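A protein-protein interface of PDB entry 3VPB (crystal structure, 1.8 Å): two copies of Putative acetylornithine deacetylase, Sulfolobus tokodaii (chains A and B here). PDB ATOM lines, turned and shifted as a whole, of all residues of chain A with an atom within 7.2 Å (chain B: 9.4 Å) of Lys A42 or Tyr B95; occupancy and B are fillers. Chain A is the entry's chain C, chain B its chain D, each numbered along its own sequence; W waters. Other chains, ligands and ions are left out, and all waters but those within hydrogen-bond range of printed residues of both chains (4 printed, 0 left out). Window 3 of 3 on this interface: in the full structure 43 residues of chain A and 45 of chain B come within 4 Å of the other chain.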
ATOM      1  N   PRO A  39     -27.430  15.755  29.530  1.00  0.00           N
ATOM      2  CA  PRO A  39     -26.670  15.537  28.307  1.00  0.00           C
ATOM      3  C   PRO A  39     -25.615  16.611  28.095  1.00  0.00           C
ATOM      4  O   PRO A  39     -25.770  17.728  28.606  1.00  0.00           O
ATOM      5  CB  PRO A  39     -27.744  15.618  27.225  1.00  0.00           C
ATOM      6  CG  PRO A  39     -28.744  16.632  27.776  1.00  0.00           C
ATOM      7  CD  PRO A  39     -28.764  16.355  29.274  1.00  0.00           C
ATOM      8  N   PHE A  40     -24.539  16.267  27.376  1.00  0.00           N
ATOM      9  CA  PHE A  40     -23.616  17.278  26.851  1.00  0.00           C
ATOM     10  C   PHE A  40     -24.238  17.736  25.562  1.00  0.00           C
ATOM     11  O   PHE A  40     -24.038  17.125  24.503  1.00  0.00           O
ATOM     12  CB  PHE A  40     -22.224  16.699  26.536  1.00  0.00           C
ATOM     13  CG  PHE A  40     -21.284  16.685  27.694  1.00  0.00           C
ATOM     14  CD1 PHE A  40     -20.923  15.493  28.296  1.00  0.00           C
ATOM     15  CD2 PHE A  40     -20.753  17.875  28.201  1.00  0.00           C
ATOM     16  CE1 PHE A  40     -20.026  15.470  29.373  1.00  0.00           C
ATOM     17  CE2 PHE A  40     -19.863  17.853  29.287  1.00  0.00           C
ATOM     18  CZ  PHE A  40     -19.507  16.637  29.878  1.00  0.00           C
ATOM     19  N   ASN A  41     -25.036  18.788  25.656  1.00  0.00           N
ATOM     20  CA  ASN A  41     -25.481  19.488  24.467  1.00  0.00           C
ATOM     21  C   ASN A  41     -25.766  20.938  24.823  1.00  0.00           C
ATOM     22  O   ASN A  41     -25.323  21.421  25.871  1.00  0.00           O
ATOM     23  CB  ASN A  41     -26.654  18.778  23.765  1.00  0.00           C
ATOM     24  CG  ASN A  41     -27.891  18.684  24.623  1.00  0.00           C
ATOM     25  OD1 ASN A  41     -28.102  19.493  25.529  1.00  0.00           O
ATOM     26  ND2 ASN A  41     -28.733  17.694  24.331  1.00  0.00           N
ATOM     27  N   LYS A  42     -26.476  21.640  23.959  1.00  0.00           N
ATOM     28  CA  LYS A  42     -26.650  23.068  24.142  1.00  0.00           C
ATOM     29  C   LYS A  42     -27.981  23.443  24.813  1.00  0.00           C
ATOM     30  O   LYS A  42     -28.232  24.618  25.054  1.00  0.00           O
ATOM     31  CB  LYS A  42     -26.441  23.799  22.811  1.00  0.00           C
ATOM     32  CG  LYS A  42     -24.958  24.026  22.468  1.00  0.00           C
ATOM     33  CD  LYS A  42     -24.695  24.296  20.968  1.00  0.00           C
ATOM     34  CE  LYS A  42     -25.541  25.452  20.384  1.00  0.00           C
ATOM     35  NZ  LYS A  42     -25.226  26.790  20.977  1.00  0.00           N
ATOM     36  N   ALA A  43     -28.798  22.438  25.147  1.00  0.00           N
ATOM     37  CA  ALA A  43     -30.092  22.642  25.815  1.00  0.00           C
ATOM     38  C   ALA A  43     -30.010  23.479  27.100  1.00  0.00           C
ATOM     39  O   ALA A  43     -30.746  24.463  27.250  1.00  0.00           O
ATOM     40  CB  ALA A  43     -30.775  21.288  26.108  1.00  0.00           C
ATOM     41  N   LEU A  44     -29.105  23.093  28.004  1.00  0.00           N
ATOM     42  CA  LEU A  44     -28.949  23.733  29.317  1.00  0.00           C
ATOM     43  C   LEU A  44     -28.521  25.202  29.227  1.00  0.00           C
ATOM     44  O   LEU A  44     -28.572  25.937  30.213  1.00  0.00           O
ATOM     45  CB  LEU A  44     -27.988  22.928  30.215  1.00  0.00           C
ATOM     46  CG  LEU A  44     -28.456  21.547  30.757  1.00  0.00           C
ATOM     47  CD1 LEU A  44     -27.337  20.801  31.481  1.00  0.00           C
ATOM     48  CD2 LEU A  44     -29.677  21.630  31.667  1.00  0.00           C
ATOM     49  N   GLY A  45     -28.126  25.629  28.034  1.00  0.00           N
ATOM     50  CA  GLY A  45     -27.730  27.013  27.781  1.00  0.00           C
ATOM     51  C   GLY A  45     -28.829  28.042  27.979  1.00  0.00           C
ATOM     52  O   GLY A  45     -28.564  29.246  27.963  1.00  0.00           O
ATOM     53  N   ARG A  46     -30.055  27.568  28.181  1.00  0.00           N
ATOM     54  CA  ARG A  46     -31.217  28.431  28.467  1.00  0.00           C
ATOM     55  C   ARG A  46     -31.079  29.108  29.845  1.00  0.00           C
ATOM     56  O   ARG A  46     -31.657  30.176  30.086  1.00  0.00           O
ATOM     57  CB  ARG A  46     -32.517  27.617  28.382  1.00  0.00           C
ATOM     58  CG  ARG A  46     -32.843  26.807  29.654  1.00  0.00           C
ATOM     59  CD  ARG A  46     -33.981  25.819  29.471  1.00  0.00           C
ATOM     60  NE  ARG A  46     -33.511  24.600  28.830  1.00  0.00           N
ATOM     61  CZ  ARG A  46     -33.516  23.391  29.387  1.00  0.00           C
ATOM     62  NH1 ARG A  46     -33.997  23.208  30.611  1.00  0.00           N
ATOM     63  NH2 ARG A  46     -33.054  22.357  28.705  1.00  0.00           N
ATOM     64  N   TYR A  47     -30.300  28.484  30.734  1.00  0.00           N
ATOM     65  CA  TYR A  47     -29.993  29.051  32.059  1.00  0.00           C
ATOM     66  C   TYR A  47     -28.831  30.025  32.048  1.00  0.00           C
ATOM     67  O   TYR A  47     -27.813  29.780  31.409  1.00  0.00           O
ATOM     68  CB  TYR A  47     -29.743  27.915  33.055  1.00  0.00           C
ATOM     69  CG  TYR A  47     -30.936  27.011  33.145  1.00  0.00           C
ATOM     70  CD1 TYR A  47     -32.148  27.491  33.643  1.00  0.00           C
ATOM     71  CD2 TYR A  47     -30.872  25.692  32.717  1.00  0.00           C
ATOM     72  CE1 TYR A  47     -33.258  26.676  33.725  1.00  0.00           C
ATOM     73  CE2 TYR A  47     -31.976  24.871  32.781  1.00  0.00           C
ATOM     74  CZ  TYR A  47     -33.173  25.380  33.294  1.00  0.00           C
ATOM     75  OH  TYR A  47     -34.276  24.578  33.374  1.00  0.00           O
ATOM     76  N   VAL A  66     -21.021  19.653  33.393  1.00  0.00           N
ATOM     77  CA  VAL A  66     -21.964  19.554  32.261  1.00  0.00           C
ATOM     78  C   VAL A  66     -22.623  20.910  31.954  1.00  0.00           C
ATOM     79  O   VAL A  66     -22.778  21.285  30.796  1.00  0.00           O
ATOM     80  CB  VAL A  66     -23.024  18.434  32.469  1.00  0.00           C
ATOM     81  CG1 VAL A  66     -24.054  18.415  31.309  1.00  0.00           C
ATOM     82  CG2 VAL A  66     -22.343  17.100  32.569  1.00  0.00           C
ATOM     83  N   GLU A  68     -21.416  23.915  32.665  1.00  0.00           N
ATOM     84  CA  GLU A  68     -20.373  24.783  32.103  1.00  0.00           C
ATOM     85  C   GLU A  68     -20.124  24.502  30.626  1.00  0.00           C
ATOM     86  O   GLU A  68     -19.826  25.419  29.854  1.00  0.00           O
ATOM     87  CB  GLU A  68     -19.053  24.594  32.849  1.00  0.00           C
ATOM     88  CG  GLU A  68     -19.050  25.194  34.210  1.00  0.00           C
ATOM     89  CD  GLU A  68     -17.795  24.804  34.986  1.00  0.00           C
ATOM     90  OE1 GLU A  68     -17.567  25.397  36.040  1.00  0.00           O
ATOM     91  OE2 GLU A  68     -17.028  23.925  34.523  1.00  0.00           O
ATOM     92  N   ALA A  69     -20.214  23.236  30.241  1.00  0.00           N
ATOM     93  CA  ALA A  69     -20.046  22.837  28.839  1.00  0.00           C
ATOM     94  C   ALA A  69     -21.090  23.499  27.932  1.00  0.00           C
ATOM     95  O   ALA A  69     -20.796  23.828  26.767  1.00  0.00           O
ATOM     96  CB  ALA A  69     -20.115  21.333  28.704  1.00  0.00           C
ATOM     97  N   ALA A  70     -22.274  23.727  28.496  1.00  0.00           N
ATOM     98  CA  ALA A  70     -23.392  24.378  27.811  1.00  0.00           C
ATOM     99  C   ALA A  70     -23.310  25.904  27.874  1.00  0.00           C
ATOM    100  O   ALA A  70     -24.190  26.589  27.354  1.00  0.00           O
ATOM    101  CB  ALA A  70     -24.711  23.902  28.388  1.00  0.00           C
ATOM    102  N   GLY A  71     -22.277  26.422  28.532  1.00  0.00           N
ATOM    103  CA  GLY A  71     -22.084  27.881  28.680  1.00  0.00           C
ATOM    104  C   GLY A  71     -22.790  28.536  29.870  1.00  0.00           C
ATOM    105  O   GLY A  71     -22.839  29.772  29.975  1.00  0.00           O
ATOM    106  N   LYS B  87     -12.755  11.858  32.769  1.00  0.00           N
ATOM    107  CA  LYS B  87     -13.393  11.943  31.447  1.00  0.00           C
ATOM    108  C   LYS B  87     -14.464  13.030  31.321  1.00  0.00           C
ATOM    109  O   LYS B  87     -14.549  13.731  30.300  1.00  0.00           O
ATOM    110  CB  LYS B  87     -13.940  10.571  31.002  1.00  0.00           C
ATOM    111  CG  LYS B  87     -12.816   9.560  30.654  1.00  0.00           C
ATOM    112  CD  LYS B  87     -13.350   8.491  29.729  1.00  0.00           C
ATOM    113  CE  LYS B  87     -12.224   7.588  29.301  1.00  0.00           C
ATOM    114  NZ  LYS B  87     -11.681   6.860  30.483  1.00  0.00           N
ATOM    115  N   ILE B  88     -15.250  13.210  32.380  1.00  0.00           N
ATOM    116  CA  ILE B  88     -16.313  14.202  32.384  1.00  0.00           C
ATOM    117  C   ILE B  88     -15.729  15.607  32.352  1.00  0.00           C
ATOM    118  O   ILE B  88     -16.180  16.452  31.556  1.00  0.00           O
ATOM    119  CB  ILE B  88     -17.262  13.983  33.585  1.00  0.00           C
ATOM    120  CG1 ILE B  88     -18.004  12.657  33.377  1.00  0.00           C
ATOM    121  CG2 ILE B  88     -18.237  15.155  33.768  1.00  0.00           C
ATOM    122  CD1 ILE B  88     -18.871  12.218  34.618  1.00  0.00           C
ATOM    123  N   LEU B  89     -14.709  15.852  33.189  1.00  0.00           N
ATOM    124  CA  LEU B  89     -14.046  17.164  33.178  1.00  0.00           C
ATOM    125  C   LEU B  89     -13.394  17.455  31.828  1.00  0.00           C
ATOM    126  O   LEU B  89     -13.455  18.599  31.340  1.00  0.00           O
ATOM    127  CB  LEU B  89     -13.000  17.279  34.314  1.00  0.00           C
ATOM    128  CG  LEU B  89     -13.552  17.116  35.742  1.00  0.00           C
ATOM    129  CD1 LEU B  89     -12.521  17.433  36.779  1.00  0.00           C
ATOM    130  CD2 LEU B  89     -14.827  17.942  35.973  1.00  0.00           C
ATOM    131  N   THR B  90     -12.743  16.438  31.253  1.00  0.00           N
ATOM    132  CA  THR B  90     -12.206  16.548  29.896  1.00  0.00           C
ATOM    133  C   THR B  90     -13.286  16.865  28.853  1.00  0.00           C
ATOM    134  O   THR B  90     -13.191  17.855  28.122  1.00  0.00           O
ATOM    135  CB  THR B  90     -11.437  15.281  29.467  1.00  0.00           C
ATOM    136  OG1 THR B  90     -10.374  15.025  30.396  1.00  0.00           O
ATOM    137  CG2 THR B  90     -10.848  15.481  28.055  1.00  0.00           C
ATOM    138  N   TYR B  91     -14.306  16.026  28.769  1.00  0.00           N
ATOM    139  CA  TYR B  91     -15.394  16.280  27.819  1.00  0.00           C
ATOM    140  C   TYR B  91     -15.998  17.689  27.963  1.00  0.00           C
ATOM    141  O   TYR B  91     -16.274  18.365  26.943  1.00  0.00           O
ATOM    142  CB  TYR B  91     -16.489  15.234  27.941  1.00  0.00           C
ATOM    143  CG  TYR B  91     -16.097  13.868  27.451  1.00  0.00           C
ATOM    144  CD1 TYR B  91     -16.548  12.732  28.122  1.00  0.00           C
ATOM    145  CD2 TYR B  91     -15.308  13.687  26.308  1.00  0.00           C
ATOM    146  CE1 TYR B  91     -16.224  11.456  27.684  1.00  0.00           C
ATOM    147  CE2 TYR B  91     -14.960  12.383  25.860  1.00  0.00           C
ATOM    148  CZ  TYR B  91     -15.434  11.284  26.567  1.00  0.00           C
ATOM    149  OH  TYR B  91     -15.124   9.992  26.191  1.00  0.00           O
ATOM    150  N   SER B  92     -16.170  18.132  29.205  1.00  0.00           N
ATOM    151  CA  SER B  92     -16.712  19.470  29.464  1.00  0.00           C
ATOM    152  C   SER B  92     -15.857  20.573  28.804  1.00  0.00           C
ATOM    153  O   SER B  92     -16.396  21.468  28.139  1.00  0.00           O
ATOM    154  CB  SER B  92     -16.837  19.733  30.967  1.00  0.00           C
ATOM    155  OG  SER B  92     -17.252  21.080  31.182  1.00  0.00           O
ATOM    156  N   LYS B  93     -14.537  20.515  28.980  1.00  0.00           N
ATOM    157  CA  LYS B  93     -13.656  21.544  28.379  1.00  0.00           C
ATOM    158  C   LYS B  93     -13.670  21.469  26.854  1.00  0.00           C
ATOM    159  O   LYS B  93     -13.697  22.505  26.166  1.00  0.00           O
ATOM    160  CB  LYS B  93     -12.214  21.441  28.916  1.00  0.00           C
ATOM    161  CG  LYS B  93     -12.130  21.731  30.387  1.00  0.00           C
ATOM    162  CD  LYS B  93     -10.757  22.145  30.831  1.00  0.00           C
ATOM    163  CE  LYS B  93     -10.905  22.998  32.086  1.00  0.00           C
ATOM    164  NZ  LYS B  93      -9.811  23.999  32.184  1.00  0.00           N
ATOM    165  N   LEU B  94     -13.663  20.245  26.320  1.00  0.00           N
ATOM    166  CA  LEU B  94     -13.605  20.053  24.868  1.00  0.00           C
ATOM    167  C   LEU B  94     -14.904  20.506  24.203  1.00  0.00           C
ATOM    168  O   LEU B  94     -14.905  21.238  23.189  1.00  0.00           O
ATOM    169  CB  LEU B  94     -13.301  18.597  24.537  1.00  0.00           C
ATOM    170  CG  LEU B  94     -11.981  18.041  25.085  1.00  0.00           C
ATOM    171  CD1 LEU B  94     -11.911  16.539  24.692  1.00  0.00           C
ATOM    172  CD2 LEU B  94     -10.749  18.775  24.606  1.00  0.00           C
ATOM    173  N   TYR B  95     -16.021  20.130  24.818  1.00  0.00           N
ATOM    174  CA  TYR B  95     -17.331  20.429  24.241  1.00  0.00           C
ATOM    175  C   TYR B  95     -17.587  21.957  24.198  1.00  0.00           C
ATOM    176  O   TYR B  95     -18.100  22.479  23.210  1.00  0.00           O
ATOM    177  CB  TYR B  95     -18.447  19.696  25.001  1.00  0.00           C
ATOM    178  CG  TYR B  95     -19.791  19.849  24.344  1.00  0.00           C
ATOM    179  CD1 TYR B  95     -20.199  18.980  23.325  1.00  0.00           C
ATOM    180  CD2 TYR B  95     -20.631  20.914  24.690  1.00  0.00           C
ATOM    181  CE1 TYR B  95     -21.439  19.157  22.701  1.00  0.00           C
ATOM    182  CE2 TYR B  95     -21.857  21.088  24.074  1.00  0.00           C
ATOM    183  CZ  TYR B  95     -22.248  20.218  23.081  1.00  0.00           C
ATOM    184  OH  TYR B  95     -23.465  20.419  22.477  1.00  0.00           O
ATOM    185  N   ARG B  96     -17.262  22.630  25.292  1.00  0.00           N
ATOM    186  CA  ARG B  96     -17.372  24.091  25.410  1.00  0.00           C
ATOM    187  C   ARG B  96     -16.603  24.807  24.304  1.00  0.00           C
ATOM    188  O   ARG B  96     -17.023  25.861  23.826  1.00  0.00           O
ATOM    189  CB  ARG B  96     -16.842  24.545  26.773  1.00  0.00           C
ATOM    190  CG  ARG B  96     -17.321  25.921  27.214  1.00  0.00           C
ATOM    191  CD  ARG B  96     -16.341  26.554  28.206  1.00  0.00           C
ATOM    192  NE  ARG B  96     -16.020  25.680  29.343  1.00  0.00           N
ATOM    193  CZ  ARG B  96     -14.843  25.665  29.972  1.00  0.00           C
ATOM    194  NH1 ARG B  96     -13.865  26.467  29.581  1.00  0.00           N
ATOM    195  NH2 ARG B  96     -14.633  24.841  30.995  1.00  0.00           N
ATOM    196  N   GLU B  97     -15.484  24.221  23.892  1.00  0.00           N
ATOM    197  CA  GLU B  97     -14.656  24.809  22.839  1.00  0.00           C
ATOM    198  C   GLU B  97     -15.003  24.370  21.412  1.00  0.00           C
ATOM    199  O   GLU B  97     -14.431  24.888  20.459  1.00  0.00           O
ATOM    200  CB  GLU B  97     -13.177  24.559  23.136  1.00  0.00           C
ATOM    201  CG  GLU B  97     -12.668  25.208  24.422  1.00  0.00           C
ATOM    202  CD  GLU B  97     -12.815  26.725  24.452  1.00  0.00           C
ATOM    203  OE1 GLU B  97     -13.298  27.248  25.486  1.00  0.00           O
ATOM    204  OE2 GLU B  97     -12.453  27.391  23.451  1.00  0.00           O
ATOM    205  N   GLY B  98     -15.941  23.435  21.260  1.00  0.00           N
ATOM    206  CA  GLY B  98     -16.386  22.984  19.938  1.00  0.00           C
ATOM    207  C   GLY B  98     -15.530  21.879  19.338  1.00  0.00           C
ATOM    208  O   GLY B  98     -15.573  21.650  18.128  1.00  0.00           O
ATOM    209  N   ILE B  99     -14.757  21.197  20.187  1.00  0.00           N
ATOM    210  CA  ILE B  99     -13.983  20.010  19.797  1.00  0.00           C
ATOM    211  C   ILE B  99     -14.899  18.791  19.856  1.00  0.00           C
ATOM    212  O   ILE B  99     -15.526  18.565  20.898  1.00  0.00           O
ATOM    213  CB  ILE B  99     -12.772  19.773  20.764  1.00  0.00           C
ATOM    214  CG1 ILE B  99     -11.876  21.012  20.857  1.00  0.00           C
ATOM    215  CG2 ILE B  99     -11.943  18.568  20.320  1.00  0.00           C
ATOM    216  CD1 ILE B  99     -11.267  21.424  19.566  1.00  0.00           C
ATOM    217  N   PRO B 100     -15.023  18.038  18.742  1.00  0.00           N
ATOM    218  CA  PRO B 100     -15.973  16.914  18.704  1.00  0.00           C
ATOM    219  C   PRO B 100     -15.619  15.854  19.743  1.00  0.00           C
ATOM    220  O   PRO B 100     -14.440  15.530  19.939  1.00  0.00           O
ATOM    221  CB  PRO B 100     -15.790  16.329  17.290  1.00  0.00           C
ATOM    222  CG  PRO B 100     -15.324  17.497  16.476  1.00  0.00           C
ATOM    223  CD  PRO B 100     -14.401  18.266  17.426  1.00  0.00           C
ATOM    224  N   ILE B 101     -16.648  15.365  20.422  1.00  0.00           N
ATOM    225  CA  ILE B 101     -16.506  14.259  21.380  1.00  0.00           C
ATOM    226  C   ILE B 101     -17.594  13.256  21.049  1.00  0.00           C
ATOM    227  O   ILE B 101     -18.515  13.596  20.339  1.00  0.00           O
ATOM    228  CB  ILE B 101     -16.650  14.762  22.866  1.00  0.00           C
ATOM    229  CG1 ILE B 101     -18.034  15.406  23.120  1.00  0.00           C
ATOM    230  CG2 ILE B 101     -15.466  15.671  23.247  1.00  0.00           C
ATOM    231  CD1 ILE B 101     -18.305  15.690  24.617  1.00  0.00           C
ATOM    232  N   PRO B 102     -17.512  12.013  21.567  1.00  0.00           N
ATOM    233  CA  PRO B 102     -18.661  11.137  21.323  1.00  0.00           C
ATOM    234  C   PRO B 102     -19.900  11.756  21.960  1.00  0.00           C
ATOM    235  O   PRO B 102     -19.784  12.375  23.026  1.00  0.00           O
ATOM    236  CB  PRO B 102     -18.296   9.842  22.072  1.00  0.00           C
ATOM    237  CG  PRO B 102     -16.834   9.852  22.192  1.00  0.00           C
ATOM    238  CD  PRO B 102     -16.433  11.335  22.312  1.00  0.00           C
ATOM    239  N   ASP B 103     -21.061  11.581  21.329  1.00  0.00           N
ATOM    240  CA  ASP B 103     -22.331  12.068  21.897  1.00  0.00           C
ATOM    241  C   ASP B 103     -22.530  11.403  23.262  1.00  0.00           C
ATOM    242  O   ASP B 103     -22.551  10.168  23.351  1.00  0.00           O
ATOM    243  CB  ASP B 103     -23.518  11.752  20.970  1.00  0.00           C
ATOM    244  CG  ASP B 103     -23.539  12.621  19.703  1.00  0.00           C
ATOM    245  OD1 ASP B 103     -22.944  13.729  19.697  1.00  0.00           O
ATOM    246  OD2 ASP B 103     -24.181  12.192  18.714  1.00  0.00           O
ATOM    247  N   SER B 104     -22.656  12.208  24.318  1.00  0.00           N
ATOM    248  CA  SER B 104     -22.565  11.713  25.688  1.00  0.00           C
ATOM    249  C   SER B 104     -23.675  12.253  26.592  1.00  0.00           C
ATOM    250  O   SER B 104     -24.025  13.410  26.508  1.00  0.00           O
ATOM    251  CB  SER B 104     -21.223  12.113  26.318  1.00  0.00           C
ATOM    252  OG  SER B 104     -20.145  11.495  25.652  1.00  0.00           O
ATOM    253  N   ALA B 225      -7.187  20.193  21.154  1.00  0.00           N
ATOM    254  CA  ALA B 225      -7.551  19.534  22.412  1.00  0.00           C
ATOM    255  C   ALA B 225      -6.481  19.679  23.483  1.00  0.00           C
ATOM    256  O   ALA B 225      -6.789  19.998  24.635  1.00  0.00           O
ATOM    257  CB  ALA B 225      -7.864  18.050  22.174  1.00  0.00           C
ATOM    258  N   ILE B 228      -6.400  23.376  24.860  1.00  0.00           N
ATOM    259  CA  ILE B 228      -7.538  23.630  25.752  1.00  0.00           C
ATOM    260  C   ILE B 228      -7.292  23.112  27.180  1.00  0.00           C
ATOM    261  O   ILE B 228      -7.668  23.777  28.151  1.00  0.00           O
ATOM    262  CB  ILE B 228      -8.831  23.023  25.152  1.00  0.00           C
ATOM    263  CG1 ILE B 228      -9.343  23.955  24.056  1.00  0.00           C
ATOM    264  CG2 ILE B 228      -9.908  22.831  26.226  1.00  0.00           C
ATOM    265  CD1 ILE B 228     -10.064  23.286  22.896  1.00  0.00           C
ATOM    266  N   VAL B 229      -6.638  21.957  27.314  1.00  0.00           N
ATOM    267  CA  VAL B 229      -6.381  21.413  28.659  1.00  0.00           C
ATOM    268  C   VAL B 229      -5.024  21.850  29.238  1.00  0.00           C
ATOM    269  O   VAL B 229      -4.727  21.609  30.418  1.00  0.00           O
ATOM    270  CB  VAL B 229      -6.620  19.869  28.761  1.00  0.00           C
ATOM    271  CG1 VAL B 229      -8.061  19.510  28.352  1.00  0.00           C
ATOM    272  CG2 VAL B 229      -5.609  19.069  27.920  1.00  0.00           C
ATOM    273  N   LYS B 244     -18.980  12.485  12.147  1.00  0.00           N
ATOM    274  CA  LYS B 244     -18.316  13.579  12.833  1.00  0.00           C
ATOM    275  C   LYS B 244     -16.853  13.728  12.439  1.00  0.00           C
ATOM    276  O   LYS B 244     -16.229  14.763  12.710  1.00  0.00           O
ATOM    277  CB  LYS B 244     -18.397  13.369  14.345  1.00  0.00           C
ATOM    278  CG  LYS B 244     -19.801  13.362  14.887  1.00  0.00           C
ATOM    279  CD  LYS B 244     -19.766  13.101  16.368  1.00  0.00           C
ATOM    280  CE  LYS B 244     -19.484  14.362  17.140  1.00  0.00           C
ATOM    281  NZ  LYS B 244     -20.078  14.178  18.477  1.00  0.00           N
ATOM    282  N   VAL B 248     -12.617  13.321  19.933  1.00  0.00           N
ATOM    283  CA  VAL B 248     -11.666  13.104  21.007  1.00  0.00           C
ATOM    284  C   VAL B 248     -12.366  12.311  22.099  1.00  0.00           C
ATOM    285  O   VAL B 248     -13.417  12.738  22.623  1.00  0.00           O
ATOM    286  CB  VAL B 248     -11.106  14.439  21.534  1.00  0.00           C
ATOM    287  CG1 VAL B 248     -10.095  14.182  22.658  1.00  0.00           C
ATOM    288  CG2 VAL B 248     -10.508  15.208  20.391  1.00  0.00           C
HETATM  289  O   HOH W   1     -15.732  22.933  32.387  1.00  0.00           O
HETATM  290  O   HOH W   2     -26.516  20.547  20.997  1.00  0.00           O
HETATM  291  O   HOH W   3     -22.136  14.929  23.689  1.00  0.00           O
HETATM  292  O   HOH W   4     -18.584  27.743  30.219  1.00  0.00           O
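N of Ala A43 is in hydrogen-bond range of OD1 of Asn A41 (3.1 Å).
The backbone carbonyl oxygen (O) of Pro B102 sits at hydrogen-bond distance from the side-chain hydroxyl (OG) of Ser B104.
The backbone NH (N) of Phe A40 is in hydrogen-bond range of the backbone carbonyl oxygen (O) of Ser B104.
CA of Pro A39 touches O of Ser B104, at 3.8 Å.
Phe A40 touches Ile B88 (CZ to O, 3.7 Å).
CE1 of Phe A40 touches CB of Tyr B91, 3.8 Å away.
Ser B92 touches Phe A40 (CA to CE2, 3.5 Å).
CE1 of Tyr B95 touches O of Phe A40, 3.8 Å away.
Lys A42 touches Tyr B95.
Arg B96 touches Glu A68 (CG to O, 3.7 Å).
Ser B92 touches Ala A69.
Ala A69 touches Tyr B95.
Ala A69 touches Arg B96 (O to CA, 3.7 Å).
Printed residues of chain B within 4 Å of Pro A39: Ser B104 (3.8 Å).
Of the printed residues of chain B, Asn A41 touches Tyr B95.
Of chain B, only Tyr B95 (3.6 Å) comes within 4 Å of Lys A42.
Printed residues of chain B within 4 Å of Glu A68: Arg B96 (3.7 Å).
Printed residues of chain B within 4 Å of Ala A69: Ser B92 (3.8 Å), Tyr B95 (3.6 Å) and Arg B96 (3.7 Å).
Printed residues of chain A within 4 Å of Ser B92: Phe A40 and Ala A69.
Lys B93 touches none of the printed residues of chain A.
Of the printed residues of chain A, Tyr B95 touches Phe A40, Asn A41, Lys A42 and Ala A69.
Of the printed residues of chain A, Arg B96 touches Glu A68 (3.7 Å) and Ala A69 (3.7 Å).
The nearest residue of chain A that does not touch Tyr B95 is Ala A70 (5.0 Å).
Water W1 lies within hydrogen-bond range of NH2 of Arg B96, OG of Ser B92 and OE2 of Glu A68.
Water W4 lies within hydrogen-bond range of the backbone carbonyl oxygen (O) of Glu A68 and the guanidinium group (NE) of Arg B96.
Water W3 lies within hydrogen-bond range of N of Ser B104 (2.8 Å) and O of Phe A40 (3.0 Å).
Water W2 bridges the backbone NH (N) of Lys A42 and the side-chain hydroxyl (OH) of Tyr B95.
No position is printed for both chains.
Of the 14 printed residues of chain A, 6 touch a printed residue of chain B.
Hydrophobic or aromatic side chains of chain B that line the printed part of chain A: Tyr B91 and Tyr B95.
Among the printed residues, 12 pairs touch across the chains.
Among the printed residues, no Asp or Glu carboxylate lies within 4 Å of a Lys or Arg side-chain nitrogen of the other chain.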
